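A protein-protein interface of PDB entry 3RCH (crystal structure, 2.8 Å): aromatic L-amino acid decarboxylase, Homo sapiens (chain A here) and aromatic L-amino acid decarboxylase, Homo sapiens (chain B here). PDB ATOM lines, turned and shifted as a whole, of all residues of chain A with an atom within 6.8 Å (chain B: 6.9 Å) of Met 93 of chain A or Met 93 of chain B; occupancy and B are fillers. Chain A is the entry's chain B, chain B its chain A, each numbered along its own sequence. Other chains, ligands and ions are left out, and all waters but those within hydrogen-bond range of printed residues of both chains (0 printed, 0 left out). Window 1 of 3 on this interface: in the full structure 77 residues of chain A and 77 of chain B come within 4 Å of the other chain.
OE2 of Glu 12 of chain B lies within salt-bridge range of NH1 of Arg 9 of chain B (3.0 Å).
The guanidinium group (NH1) of Arg 9 of chain A is in salt-bridge range of the side-chain carboxylate (OE1) of Glu 12 of chain A.
Among the printed residues, pairs that only touch across the chains: Phe 6 of chain A with Val 14 of chain B (3.8 Å), Phe 6 of chain A with Leu 90 of chain B (3.8 Å), Arg 9 of chain A with Leu 90 of chain B (3.6 Å), Gly 10 of chain A with Val 14 of chain B (3.7 Å), Gly 10 of chain A with Leu 90 of chain B (3.6 Å), Gly 10 of chain A with Met 93 of chain B (3.7 Å), Lys 11 of chain A with Lys 11 of chain B (3.3 Å), Lys 11 of chain A with Val 14 of chain B (3.8 Å), Met 13 of chain A with Leu 90 of chain B (3.8 Å), Met 13 of chain A with Met 93 of chain B (3.6 Å), Val 14 of chain A with Phe 6 of chain B (3.8 Å), Val 14 of chain A with Gly 10 of chain B (3.6 Å), Val 14 of chain A with Lys 11 of chain B (3.8 Å), Val 14 of chain A with Val 14 of chain B (3.97 Å), Val 14 of chain A with Met 93 of chain B (3.6 Å), Val 17 of chain A with Phe 6 of chain B (3.8 Å), Val 17 of chain A with Ala 97 of chain B (3.8 Å), Met 89 of chain A with Phe 6 of chain B (3.999 Å), Met 89 of chain A with Met 93 of chain B (3.9 Å), Met 89 of chain A with Ala 97 of chain B (3.9 Å), Leu 90 of chain A with Arg 9 of chain B (3.8 Å), Leu 90 of chain A with Gly 10 of chain B (3.6 Å), Leu 90 of chain A with Met 13 of chain B (3.9 Å), Met 93 of chain A with Gly 10 of chain B (3.4 Å), Met 93 of chain A with Met 13 of chain B (3.6 Å), Met 93 of chain A with Val 14 of chain B (3.7 Å), Met 93 of chain A with Val 17 of chain B (3.9 Å), Met 93 of chain A with Met 93 of chain B (3.98 Å) and Ala 97 of chain A with Val 17 of chain B (3.7 Å).
Of the printed residues of chain B, Met 93 of chain A touches Gly 10 (3.4 Å), Met 13 (3.6 Å), Val 14 (3.7 Å), Val 17 (3.9 Å) and Met 93 (3.98 Å).
Printed residues of chain A within 4 Å of Leu 90 of chain B: Phe 6, Arg 9, Gly 10 and Met 13.
Printed residues of chain B within 4 Å of Arg 9 of chain A: Leu 90.
Of the printed residues of chain B, Asp 15 of chain A touches Lys 11.
Printed residues of chain B within 4 Å of Gly 10 of chain A: Val 14, Leu 90 and Met 93.
The nearest residue of chain B that does not touch Met 93 of chain A is Phe 6 of chain B (4.8 Å).
The nearest residue of chain A that does not touch Met 93 of chain B is Val 17 of chain A (4.1 Å).
Of the 20 printed residues of chain A, 12 touch a printed residue of chain B.
Hydrophobic or aromatic side chains of chain A that line the printed part of chain B: Phe 6, Met 13, Val 14, Val 17, Met 89, Leu 90, Met 93 and Ala 97.
Of the 20 printed residues of chain B, 11 touch a printed residue of chain A.
Printed residues of chain B that touch a printed residue of chain A: Phe 6, Arg 9, Gly 10, Lys 11, Met 13, Val 14, Asp 15, Val 17, Leu 90, Met 93 and Ala 97.
Among the printed residues, 31 pairs touch across the chains.
Among the printed residues, Asp or Glu carboxylates within 4 Å of a Lys or Arg side-chain nitrogen of the other chain: Lys 11 of chain A with Asp 15 of chain B and Asp 15 of chain A with Lys 11 of chain B.
The side-chain carboxylate (OD2) of Asp 15 of chain A is in salt-bridge range of the side-chain amino group (NZ) of Lys 11 of chain B, at 2.8 Å.
NZ of Lys 11 of chain A is in salt-bridge range of OD2 of Asp 15 of chain B.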
ATOM      1  N   PHE A   6     -25.883   3.375  -2.563  1.00  0.00           N
ATOM      2  CA  PHE A   6     -24.869   3.688  -1.582  1.00  0.00           C
ATOM      3  C   PHE A   6     -24.162   2.458  -1.005  1.00  0.00           C
ATOM      4  O   PHE A   6     -22.975   2.507  -0.716  1.00  0.00           O
ATOM      5  CB  PHE A   6     -25.406   4.616  -0.487  1.00  0.00           C
ATOM      6  CG  PHE A   6     -24.412   4.889   0.595  1.00  0.00           C
ATOM      7  CD1 PHE A   6     -23.399   5.799   0.394  1.00  0.00           C
ATOM      8  CD2 PHE A   6     -24.466   4.190   1.797  1.00  0.00           C
ATOM      9  CE1 PHE A   6     -22.476   6.029   1.375  1.00  0.00           C
ATOM     10  CE2 PHE A   6     -23.541   4.406   2.779  1.00  0.00           C
ATOM     11  CZ  PHE A   6     -22.549   5.332   2.577  1.00  0.00           C
ATOM     12  N   ARG A   9     -21.550   1.992  -4.061  1.00  0.00           N
ATOM     13  CA  ARG A   9     -20.512   3.014  -4.182  1.00  0.00           C
ATOM     14  C   ARG A   9     -19.764   3.276  -2.870  1.00  0.00           C
ATOM     15  O   ARG A   9     -18.599   3.656  -2.898  1.00  0.00           O
ATOM     16  CB  ARG A   9     -21.067   4.322  -4.753  1.00  0.00           C
ATOM     17  CG  ARG A   9     -21.850   4.211  -6.060  1.00  0.00           C
ATOM     18  CD  ARG A   9     -21.303   3.139  -6.976  1.00  0.00           C
ATOM     19  NE  ARG A   9     -21.473   3.452  -8.392  1.00  0.00           N
ATOM     20  CZ  ARG A   9     -21.342   2.556  -9.368  1.00  0.00           C
ATOM     21  NH1 ARG A   9     -21.071   1.279  -9.096  1.00  0.00           N
ATOM     22  NH2 ARG A   9     -21.503   2.933 -10.626  1.00  0.00           N
ATOM     23  N   GLY A  10     -20.439   3.064  -1.736  1.00  0.00           N
ATOM     24  CA  GLY A  10     -19.839   3.178  -0.394  1.00  0.00           C
ATOM     25  C   GLY A  10     -18.735   2.163  -0.186  1.00  0.00           C
ATOM     26  O   GLY A  10     -17.636   2.500   0.225  1.00  0.00           O
ATOM     27  N   LYS A  11     -19.012   0.910  -0.504  1.00  0.00           N
ATOM     28  CA  LYS A  11     -17.991  -0.107  -0.397  1.00  0.00           C
ATOM     29  C   LYS A  11     -16.885   0.157  -1.413  1.00  0.00           C
ATOM     30  O   LYS A  11     -15.708  -0.073  -1.132  1.00  0.00           O
ATOM     31  CB  LYS A  11     -18.607  -1.482  -0.552  1.00  0.00           C
ATOM     32  CG  LYS A  11     -19.560  -1.794   0.572  1.00  0.00           C
ATOM     33  CD  LYS A  11     -20.253  -3.110   0.362  1.00  0.00           C
ATOM     34  CE  LYS A  11     -21.056  -3.510   1.573  1.00  0.00           C
ATOM     35  NZ  LYS A  11     -22.143  -4.440   1.215  1.00  0.00           N
ATOM     36  N   GLU A  12     -17.258   0.678  -2.576  1.00  0.00           N
ATOM     37  CA  GLU A  12     -16.266   1.046  -3.580  1.00  0.00           C
ATOM     38  C   GLU A  12     -15.323   2.119  -3.042  1.00  0.00           C
ATOM     39  O   GLU A  12     -14.125   2.095  -3.323  1.00  0.00           O
ATOM     40  CB  GLU A  12     -16.934   1.537  -4.871  1.00  0.00           C
ATOM     41  CG  GLU A  12     -17.367   0.442  -5.819  1.00  0.00           C
ATOM     42  CD  GLU A  12     -18.182   0.958  -6.999  1.00  0.00           C
ATOM     43  OE1 GLU A  12     -19.329   0.492  -7.149  1.00  0.00           O
ATOM     44  OE2 GLU A  12     -17.691   1.816  -7.773  1.00  0.00           O
ATOM     45  N   MET A  13     -15.870   3.058  -2.274  1.00  0.00           N
ATOM     46  CA  MET A  13     -15.086   4.163  -1.725  1.00  0.00           C
ATOM     47  C   MET A  13     -14.171   3.672  -0.611  1.00  0.00           C
ATOM     48  O   MET A  13     -13.000   4.059  -0.554  1.00  0.00           O
ATOM     49  CB  MET A  13     -15.994   5.287  -1.234  1.00  0.00           C
ATOM     50  CG  MET A  13     -15.262   6.460  -0.603  1.00  0.00           C
ATOM     51  SD  MET A  13     -14.406   7.586  -1.722  1.00  0.00           S
ATOM     52  CE  MET A  13     -15.736   8.051  -2.830  1.00  0.00           C
ATOM     53  N   VAL A  14     -14.696   2.805   0.254  1.00  0.00           N
ATOM     54  CA  VAL A  14     -13.866   2.087   1.216  1.00  0.00           C
ATOM     55  C   VAL A  14     -12.646   1.512   0.497  1.00  0.00           C
ATOM     56  O   VAL A  14     -11.525   1.618   0.981  1.00  0.00           O
ATOM     57  CB  VAL A  14     -14.641   0.954   1.920  1.00  0.00           C
ATOM     58  CG1 VAL A  14     -13.713   0.115   2.741  1.00  0.00           C
ATOM     59  CG2 VAL A  14     -15.715   1.522   2.812  1.00  0.00           C
ATOM     60  N   ASP A  15     -12.857   0.920  -0.673  1.00  0.00           N
ATOM     61  CA  ASP A  15     -11.721   0.397  -1.420  1.00  0.00           C
ATOM     62  C   ASP A  15     -10.782   1.502  -1.887  1.00  0.00           C
ATOM     63  O   ASP A  15      -9.565   1.381  -1.734  1.00  0.00           O
ATOM     64  CB  ASP A  15     -12.158  -0.466  -2.609  1.00  0.00           C
ATOM     65  CG  ASP A  15     -12.490  -1.906  -2.209  1.00  0.00           C
ATOM     66  OD1 ASP A  15     -12.110  -2.338  -1.085  1.00  0.00           O
ATOM     67  OD2 ASP A  15     -13.143  -2.595  -3.036  1.00  0.00           O
ATOM     68  N   VAL A  17     -10.261   4.397  -0.764  1.00  0.00           N
ATOM     69  CA  VAL A  17      -9.609   5.023   0.378  1.00  0.00           C
ATOM     70  C   VAL A  17      -8.449   4.162   0.895  1.00  0.00           C
ATOM     71  O   VAL A  17      -7.342   4.667   1.077  1.00  0.00           O
ATOM     72  CB  VAL A  17     -10.633   5.363   1.489  1.00  0.00           C
ATOM     73  CG1 VAL A  17      -9.959   5.538   2.827  1.00  0.00           C
ATOM     74  CG2 VAL A  17     -11.409   6.620   1.122  1.00  0.00           C
ATOM     75  N   ALA A  88     -11.230   5.880  13.483  1.00  0.00           N
ATOM     76  CA  ALA A  88     -11.800   7.221  13.435  1.00  0.00           C
ATOM     77  C   ALA A  88     -12.672   7.430  12.204  1.00  0.00           C
ATOM     78  O   ALA A  88     -13.679   8.142  12.249  1.00  0.00           O
ATOM     79  CB  ALA A  88     -10.687   8.243  13.457  1.00  0.00           C
ATOM     80  N   MET A  89     -12.272   6.815  11.099  1.00  0.00           N
ATOM     81  CA  MET A  89     -13.002   6.926   9.849  1.00  0.00           C
ATOM     82  C   MET A  89     -14.265   6.095   9.943  1.00  0.00           C
ATOM     83  O   MET A  89     -15.323   6.483   9.437  1.00  0.00           O
ATOM     84  CB  MET A  89     -12.115   6.460   8.713  1.00  0.00           C
ATOM     85  CG  MET A  89     -10.733   7.108   8.773  1.00  0.00           C
ATOM     86  SD  MET A  89      -9.730   6.878   7.308  1.00  0.00           S
ATOM     87  CE  MET A  89     -10.961   7.330   6.077  1.00  0.00           C
ATOM     88  N   LEU A  90     -14.155   4.958  10.626  1.00  0.00           N
ATOM     89  CA  LEU A  90     -15.296   4.110  10.870  1.00  0.00           C
ATOM     90  C   LEU A  90     -16.304   4.867  11.696  1.00  0.00           C
ATOM     91  O   LEU A  90     -17.486   4.870  11.371  1.00  0.00           O
ATOM     92  CB  LEU A  90     -14.875   2.848  11.595  1.00  0.00           C
ATOM     93  CG  LEU A  90     -14.189   1.779  10.757  1.00  0.00           C
ATOM     94  CD1 LEU A  90     -13.721   0.637  11.645  1.00  0.00           C
ATOM     95  CD2 LEU A  90     -15.111   1.274   9.644  1.00  0.00           C
ATOM     96  N   ALA A  91     -15.835   5.517  12.755  1.00  0.00           N
ATOM     97  CA  ALA A  91     -16.685   6.369  13.585  1.00  0.00           C
ATOM     98  C   ALA A  91     -17.380   7.462  12.785  1.00  0.00           C
ATOM     99  O   ALA A  91     -18.596   7.636  12.894  1.00  0.00           O
ATOM    100  CB  ALA A  91     -15.875   6.985  14.712  1.00  0.00           C
ATOM    101  N   ASP A  92     -16.609   8.189  11.981  1.00  0.00           N
ATOM    102  CA  ASP A  92     -17.145   9.276  11.174  1.00  0.00           C
ATOM    103  C   ASP A  92     -18.262   8.819  10.274  1.00  0.00           C
ATOM    104  O   ASP A  92     -19.245   9.531  10.082  1.00  0.00           O
ATOM    105  CB  ASP A  92     -16.056   9.875  10.313  1.00  0.00           C
ATOM    106  CG  ASP A  92     -15.196  10.845  11.072  1.00  0.00           C
ATOM    107  OD1 ASP A  92     -15.786  11.636  11.844  1.00  0.00           O
ATOM    108  OD2 ASP A  92     -13.947  10.814  10.897  1.00  0.00           O
ATOM    109  N   MET A  93     -18.106   7.628   9.711  1.00  0.00           N
ATOM    110  CA  MET A  93     -19.101   7.115   8.812  1.00  0.00           C
ATOM    111  C   MET A  93     -20.405   6.989   9.534  1.00  0.00           C
ATOM    112  O   MET A  93     -21.427   7.375   9.013  1.00  0.00           O
ATOM    113  CB  MET A  93     -18.672   5.783   8.243  1.00  0.00           C
ATOM    114  CG  MET A  93     -17.629   5.917   7.154  1.00  0.00           C
ATOM    115  SD  MET A  93     -16.796   4.372   6.820  1.00  0.00           S
ATOM    116  CE  MET A  93     -18.175   3.339   6.369  1.00  0.00           C
ATOM    117  N   LEU A  94     -20.362   6.460  10.750  1.00  0.00           N
ATOM    118  CA  LEU A  94     -21.559   6.312  11.575  1.00  0.00           C
ATOM    119  C   LEU A  94     -22.095   7.676  11.962  1.00  0.00           C
ATOM    120  O   LEU A  94     -23.292   7.933  11.894  1.00  0.00           O
ATOM    121  CB  LEU A  94     -21.232   5.500  12.831  1.00  0.00           C
ATOM    122  CG  LEU A  94     -22.269   5.411  13.954  1.00  0.00           C
ATOM    123  CD1 LEU A  94     -23.557   4.779  13.471  1.00  0.00           C
ATOM    124  CD2 LEU A  94     -21.686   4.599  15.070  1.00  0.00           C
ATOM    125  N   CYS A  95     -21.187   8.561  12.347  1.00  0.00           N
ATOM    126  CA  CYS A  95     -21.582   9.884  12.794  1.00  0.00           C
ATOM    127  C   CYS A  95     -22.338  10.660  11.719  1.00  0.00           C
ATOM    128  O   CYS A  95     -23.216  11.466  12.026  1.00  0.00           O
ATOM    129  CB  CYS A  95     -20.386  10.659  13.315  1.00  0.00           C
ATOM    130  SG  CYS A  95     -20.697  11.195  14.990  1.00  0.00           S
ATOM    131  N   GLY A  96     -22.010  10.383  10.462  1.00  0.00           N
ATOM    132  CA  GLY A  96     -22.708  10.974   9.337  1.00  0.00           C
ATOM    133  C   GLY A  96     -24.146  10.512   9.287  1.00  0.00           C
ATOM    134  O   GLY A  96     -25.062  11.326   9.102  1.00  0.00           O
ATOM    135  N   ALA A  97     -24.344   9.206   9.462  1.00  0.00           N
ATOM    136  CA  ALA A  97     -25.670   8.597   9.369  1.00  0.00           C
ATOM    137  C   ALA A  97     -26.637   9.109  10.451  1.00  0.00           C
ATOM    138  O   ALA A  97     -27.818   9.347  10.180  1.00  0.00           O
ATOM    139  CB  ALA A  97     -25.553   7.107   9.432  1.00  0.00           C
ATOM    140  N   ILE A  98     -26.109   9.265  11.666  1.00  0.00           N
ATOM    141  CA  ILE A  98     -26.818   9.817  12.813  1.00  0.00           C
ATOM    142  C   ILE A  98     -26.937  11.334  12.678  1.00  0.00           C
ATOM    143  O   ILE A  98     -28.051  11.868  12.578  1.00  0.00           O
ATOM    144  CB  ILE A  98     -26.030   9.524  14.104  1.00  0.00           C
ATOM    145  CG1 ILE A  98     -26.180   8.066  14.514  1.00  0.00           C
ATOM    146  CG2 ILE A  98     -26.435  10.471  15.244  1.00  0.00           C
ATOM    147  CD1 ILE A  98     -25.134   7.663  15.523  1.00  0.00           C
ATOM    148  N   PHE B   6      -9.525  -2.498   7.529  1.00  0.00           N
ATOM    149  CA  PHE B   6     -10.461  -1.389   7.310  1.00  0.00           C
ATOM    150  C   PHE B   6     -11.378  -1.727   6.142  1.00  0.00           C
ATOM    151  O   PHE B   6     -12.530  -1.307   6.112  1.00  0.00           O
ATOM    152  CB  PHE B   6      -9.701  -0.070   7.042  1.00  0.00           C
ATOM    153  CG  PHE B   6     -10.586   1.096   6.621  1.00  0.00           C
ATOM    154  CD1 PHE B   6     -11.440   1.714   7.534  1.00  0.00           C
ATOM    155  CD2 PHE B   6     -10.543   1.584   5.327  1.00  0.00           C
ATOM    156  CE1 PHE B   6     -12.249   2.780   7.154  1.00  0.00           C
ATOM    157  CE2 PHE B   6     -11.342   2.644   4.941  1.00  0.00           C
ATOM    158  CZ  PHE B   6     -12.200   3.240   5.853  1.00  0.00           C
ATOM    159  N   ARG B   9     -14.177  -4.018   7.476  1.00  0.00           N
ATOM    160  CA  ARG B   9     -15.014  -3.348   8.437  1.00  0.00           C
ATOM    161  C   ARG B   9     -15.652  -2.061   7.912  1.00  0.00           C
ATOM    162  O   ARG B   9     -16.806  -1.759   8.231  1.00  0.00           O
ATOM    163  CB  ARG B   9     -14.223  -3.121   9.706  1.00  0.00           C
ATOM    164  CG  ARG B   9     -13.643  -4.405  10.246  1.00  0.00           C
ATOM    165  CD  ARG B   9     -14.733  -5.450  10.389  1.00  0.00           C
ATOM    166  NE  ARG B   9     -14.340  -6.519  11.295  1.00  0.00           N
ATOM    167  CZ  ARG B   9     -14.425  -7.808  11.013  1.00  0.00           C
ATOM    168  NH1 ARG B   9     -14.906  -8.210   9.841  1.00  0.00           N
ATOM    169  NH2 ARG B   9     -14.052  -8.700  11.912  1.00  0.00           N
ATOM    170  N   GLY B  10     -14.916  -1.314   7.097  1.00  0.00           N
ATOM    171  CA  GLY B  10     -15.499  -0.192   6.375  1.00  0.00           C
ATOM    172  C   GLY B  10     -16.725  -0.605   5.563  1.00  0.00           C
ATOM    173  O   GLY B  10     -17.798   0.012   5.671  1.00  0.00           O
ATOM    174  N   LYS B  11     -16.577  -1.655   4.761  1.00  0.00           N
ATOM    175  CA  LYS B  11     -17.687  -2.158   3.971  1.00  0.00           C
ATOM    176  C   LYS B  11     -18.815  -2.607   4.873  1.00  0.00           C
ATOM    177  O   LYS B  11     -19.978  -2.433   4.531  1.00  0.00           O
ATOM    178  CB  LYS B  11     -17.238  -3.294   3.059  1.00  0.00           C
ATOM    179  CG  LYS B  11     -16.232  -2.845   2.035  1.00  0.00           C
ATOM    180  CD  LYS B  11     -15.908  -3.873   1.028  1.00  0.00           C
ATOM    181  CE  LYS B  11     -14.866  -3.292   0.116  1.00  0.00           C
ATOM    182  NZ  LYS B  11     -15.008  -3.752  -1.296  1.00  0.00           N
ATOM    183  N   GLU B  12     -18.472  -3.168   6.035  1.00  0.00           N
ATOM    184  CA  GLU B  12     -19.479  -3.616   6.995  1.00  0.00           C
ATOM    185  C   GLU B  12     -20.272  -2.438   7.543  1.00  0.00           C
ATOM    186  O   GLU B  12     -21.499  -2.500   7.661  1.00  0.00           O
ATOM    187  CB  GLU B  12     -18.834  -4.375   8.146  1.00  0.00           C
ATOM    188  CG  GLU B  12     -18.820  -5.872   7.969  1.00  0.00           C
ATOM    189  CD  GLU B  12     -18.629  -6.608   9.287  1.00  0.00           C
ATOM    190  OE1 GLU B  12     -19.363  -6.302  10.259  1.00  0.00           O
ATOM    191  OE2 GLU B  12     -17.745  -7.495   9.341  1.00  0.00           O
ATOM    192  N   MET B  13     -19.546  -1.366   7.866  1.00  0.00           N
ATOM    193  CA  MET B  13     -20.121  -0.138   8.406  1.00  0.00           C
ATOM    194  C   MET B  13     -20.972   0.565   7.359  1.00  0.00           C
ATOM    195  O   MET B  13     -21.991   1.174   7.701  1.00  0.00           O
ATOM    196  CB  MET B  13     -19.002   0.784   8.899  1.00  0.00           C
ATOM    197  CG  MET B  13     -19.473   2.118   9.445  1.00  0.00           C
ATOM    198  SD  MET B  13     -20.416   1.942  10.968  1.00  0.00           S
ATOM    199  CE  MET B  13     -19.100   1.396  12.061  1.00  0.00           C
ATOM    200  N   VAL B  14     -20.542   0.492   6.095  1.00  0.00           N
ATOM    201  CA  VAL B  14     -21.370   0.928   4.972  1.00  0.00           C
ATOM    202  C   VAL B  14     -22.719   0.210   4.975  1.00  0.00           C
ATOM    203  O   VAL B  14     -23.756   0.836   4.788  1.00  0.00           O
ATOM    204  CB  VAL B  14     -20.675   0.722   3.596  1.00  0.00           C
ATOM    205  CG1 VAL B  14     -21.696   0.716   2.437  1.00  0.00           C
ATOM    206  CG2 VAL B  14     -19.641   1.796   3.367  1.00  0.00           C
ATOM    207  N   ASP B  15     -22.704  -1.098   5.197  1.00  0.00           N
ATOM    208  CA  ASP B  15     -23.939  -1.848   5.271  1.00  0.00           C
ATOM    209  C   ASP B  15     -24.723  -1.439   6.471  1.00  0.00           C
ATOM    210  O   ASP B  15     -25.913  -1.183   6.367  1.00  0.00           O
ATOM    211  CB  ASP B  15     -23.684  -3.345   5.324  1.00  0.00           C
ATOM    212  CG  ASP B  15     -23.650  -3.982   3.945  1.00  0.00           C
ATOM    213  OD1 ASP B  15     -24.312  -3.463   3.002  1.00  0.00           O
ATOM    214  OD2 ASP B  15     -22.947  -5.008   3.818  1.00  0.00           O
ATOM    215  N   VAL B  17     -24.743   1.338   8.060  1.00  0.00           N
ATOM    216  CA  VAL B  17     -25.307   2.651   7.782  1.00  0.00           C
ATOM    217  C   VAL B  17     -26.546   2.551   6.891  1.00  0.00           C
ATOM    218  O   VAL B  17     -27.615   3.038   7.259  1.00  0.00           O
ATOM    219  CB  VAL B  17     -24.242   3.621   7.184  1.00  0.00           C
ATOM    220  CG1 VAL B  17     -24.886   4.839   6.523  1.00  0.00           C
ATOM    221  CG2 VAL B  17     -23.272   4.058   8.259  1.00  0.00           C
ATOM    222  N   ALA B  88     -22.627  13.163  -0.075  1.00  0.00           N
ATOM    223  CA  ALA B  88     -21.763  13.902   0.843  1.00  0.00           C
ATOM    224  C   ALA B  88     -21.011  12.954   1.760  1.00  0.00           C
ATOM    225  O   ALA B  88     -19.855  13.186   2.085  1.00  0.00           O
ATOM    226  CB  ALA B  88     -22.557  14.921   1.647  1.00  0.00           C
ATOM    227  N   MET B  89     -21.682  11.887   2.169  1.00  0.00           N
ATOM    228  CA  MET B  89     -21.054  10.888   2.994  1.00  0.00           C
ATOM    229  C   MET B  89     -19.825  10.342   2.287  1.00  0.00           C
ATOM    230  O   MET B  89     -18.758  10.197   2.899  1.00  0.00           O
ATOM    231  CB  MET B  89     -22.042   9.779   3.316  1.00  0.00           C
ATOM    232  CG  MET B  89     -23.369  10.297   3.825  1.00  0.00           C
ATOM    233  SD  MET B  89     -24.374   9.000   4.560  1.00  0.00           S
ATOM    234  CE  MET B  89     -25.929   9.874   4.650  1.00  0.00           C
ATOM    235  N   LEU B  90     -19.971  10.076   0.989  1.00  0.00           N
ATOM    236  CA  LEU B  90     -18.879   9.554   0.185  1.00  0.00           C
ATOM    237  C   LEU B  90     -17.749  10.565   0.120  1.00  0.00           C
ATOM    238  O   LEU B  90     -16.580  10.198   0.183  1.00  0.00           O
ATOM    239  CB  LEU B  90     -19.354   9.193  -1.218  1.00  0.00           C
ATOM    240  CG  LEU B  90     -20.339   8.034  -1.356  1.00  0.00           C
ATOM    241  CD1 LEU B  90     -21.047   8.146  -2.683  1.00  0.00           C
ATOM    242  CD2 LEU B  90     -19.694   6.653  -1.210  1.00  0.00           C
ATOM    243  N   ALA B  91     -18.108  11.838   0.014  1.00  0.00           N
ATOM    244  CA  ALA B  91     -17.123  12.896   0.081  1.00  0.00           C
ATOM    245  C   ALA B  91     -16.426  12.944   1.447  1.00  0.00           C
ATOM    246  O   ALA B  91     -15.203  13.028   1.508  1.00  0.00           O
ATOM    247  CB  ALA B  91     -17.738  14.206  -0.251  1.00  0.00           C
ATOM    248  N   ASP B  92     -17.185  12.870   2.535  1.00  0.00           N
ATOM    249  CA  ASP B  92     -16.594  12.885   3.860  1.00  0.00           C
ATOM    250  C   ASP B  92     -15.572  11.765   3.975  1.00  0.00           C
ATOM    251  O   ASP B  92     -14.535  11.918   4.613  1.00  0.00           O
ATOM    252  CB  ASP B  92     -17.675  12.740   4.933  1.00  0.00           C
ATOM    253  CG  ASP B  92     -18.437  14.030   5.172  1.00  0.00           C
ATOM    254  OD1 ASP B  92     -17.831  15.117   5.015  1.00  0.00           O
ATOM    255  OD2 ASP B  92     -19.639  13.956   5.516  1.00  0.00           O
ATOM    256  N   MET B  93     -15.874  10.641   3.347  1.00  0.00           N
ATOM    257  CA  MET B  93     -15.003   9.494   3.444  1.00  0.00           C
ATOM    258  C   MET B  93     -13.654   9.804   2.845  1.00  0.00           C
ATOM    259  O   MET B  93     -12.624   9.736   3.519  1.00  0.00           O
ATOM    260  CB  MET B  93     -15.636   8.283   2.766  1.00  0.00           C
ATOM    261  CG  MET B  93     -16.614   7.535   3.664  1.00  0.00           C
ATOM    262  SD  MET B  93     -17.572   6.293   2.803  1.00  0.00           S
ATOM    263  CE  MET B  93     -16.311   5.041   2.570  1.00  0.00           C
ATOM    264  N   LEU B  94     -13.689  10.160   1.569  1.00  0.00           N
ATOM    265  CA  LEU B  94     -12.532  10.601   0.856  1.00  0.00           C
ATOM    266  C   LEU B  94     -11.899  11.716   1.647  1.00  0.00           C
ATOM    267  O   LEU B  94     -10.699  11.722   1.883  1.00  0.00           O
ATOM    268  CB  LEU B  94     -12.957  11.115  -0.512  1.00  0.00           C
ATOM    269  CG  LEU B  94     -11.890  11.752  -1.402  1.00  0.00           C
ATOM    270  CD1 LEU B  94     -10.784  10.771  -1.710  1.00  0.00           C
ATOM    271  CD2 LEU B  94     -12.528  12.249  -2.677  1.00  0.00           C
ATOM    272  N   CYS B  95     -12.713  12.656   2.086  1.00  0.00           N
ATOM    273  CA  CYS B  95     -12.154  13.803   2.747  1.00  0.00           C
ATOM    274  C   CYS B  95     -11.433  13.426   4.036  1.00  0.00           C
ATOM    275  O   CYS B  95     -10.484  14.081   4.424  1.00  0.00           O
ATOM    276  CB  CYS B  95     -13.210  14.865   2.977  1.00  0.00           C
ATOM    277  SG  CYS B  95     -12.520  16.504   3.176  1.00  0.00           S
ATOM    278  N   GLY B  96     -11.857  12.349   4.683  1.00  0.00           N
ATOM    279  CA  GLY B  96     -11.159  11.870   5.869  1.00  0.00           C
ATOM    280  C   GLY B  96      -9.820  11.245   5.524  1.00  0.00           C
ATOM    281  O   GLY B  96      -8.873  11.339   6.304  1.00  0.00           O
ATOM    282  N   ALA B  97      -9.746  10.599   4.358  1.00  0.00           N
ATOM    283  CA  ALA B  97      -8.502  10.001   3.855  1.00  0.00           C
ATOM    284  C   ALA B  97      -7.454  11.042   3.506  1.00  0.00           C
ATOM    285  O   ALA B  97      -6.343  10.969   3.999  1.00  0.00           O
ATOM    286  CB  ALA B  97      -8.767   9.130   2.667  1.00  0.00           C
ATOM    287  N   ILE B  98      -7.796  12.008   2.658  1.00  0.00           N
ATOM    288  CA  ILE B  98      -6.852  13.074   2.326  1.00  0.00           C
ATOM    289  C   ILE B  98      -6.461  13.867   3.580  1.00  0.00           C
ATOM    290  O   ILE B  98      -5.283  14.055   3.846  1.00  0.00           O
ATOM    291  CB  ILE B  98      -7.404  14.083   1.280  1.00  0.00           C
ATOM    292  CG1 ILE B  98      -7.901  13.403   0.014  1.00  0.00           C
ATOM    293  CG2 ILE B  98      -6.345  15.104   0.901  1.00  0.00           C
ATOM    294  CD1 ILE B  98      -8.858  14.300  -0.783  1.00  0.00           C
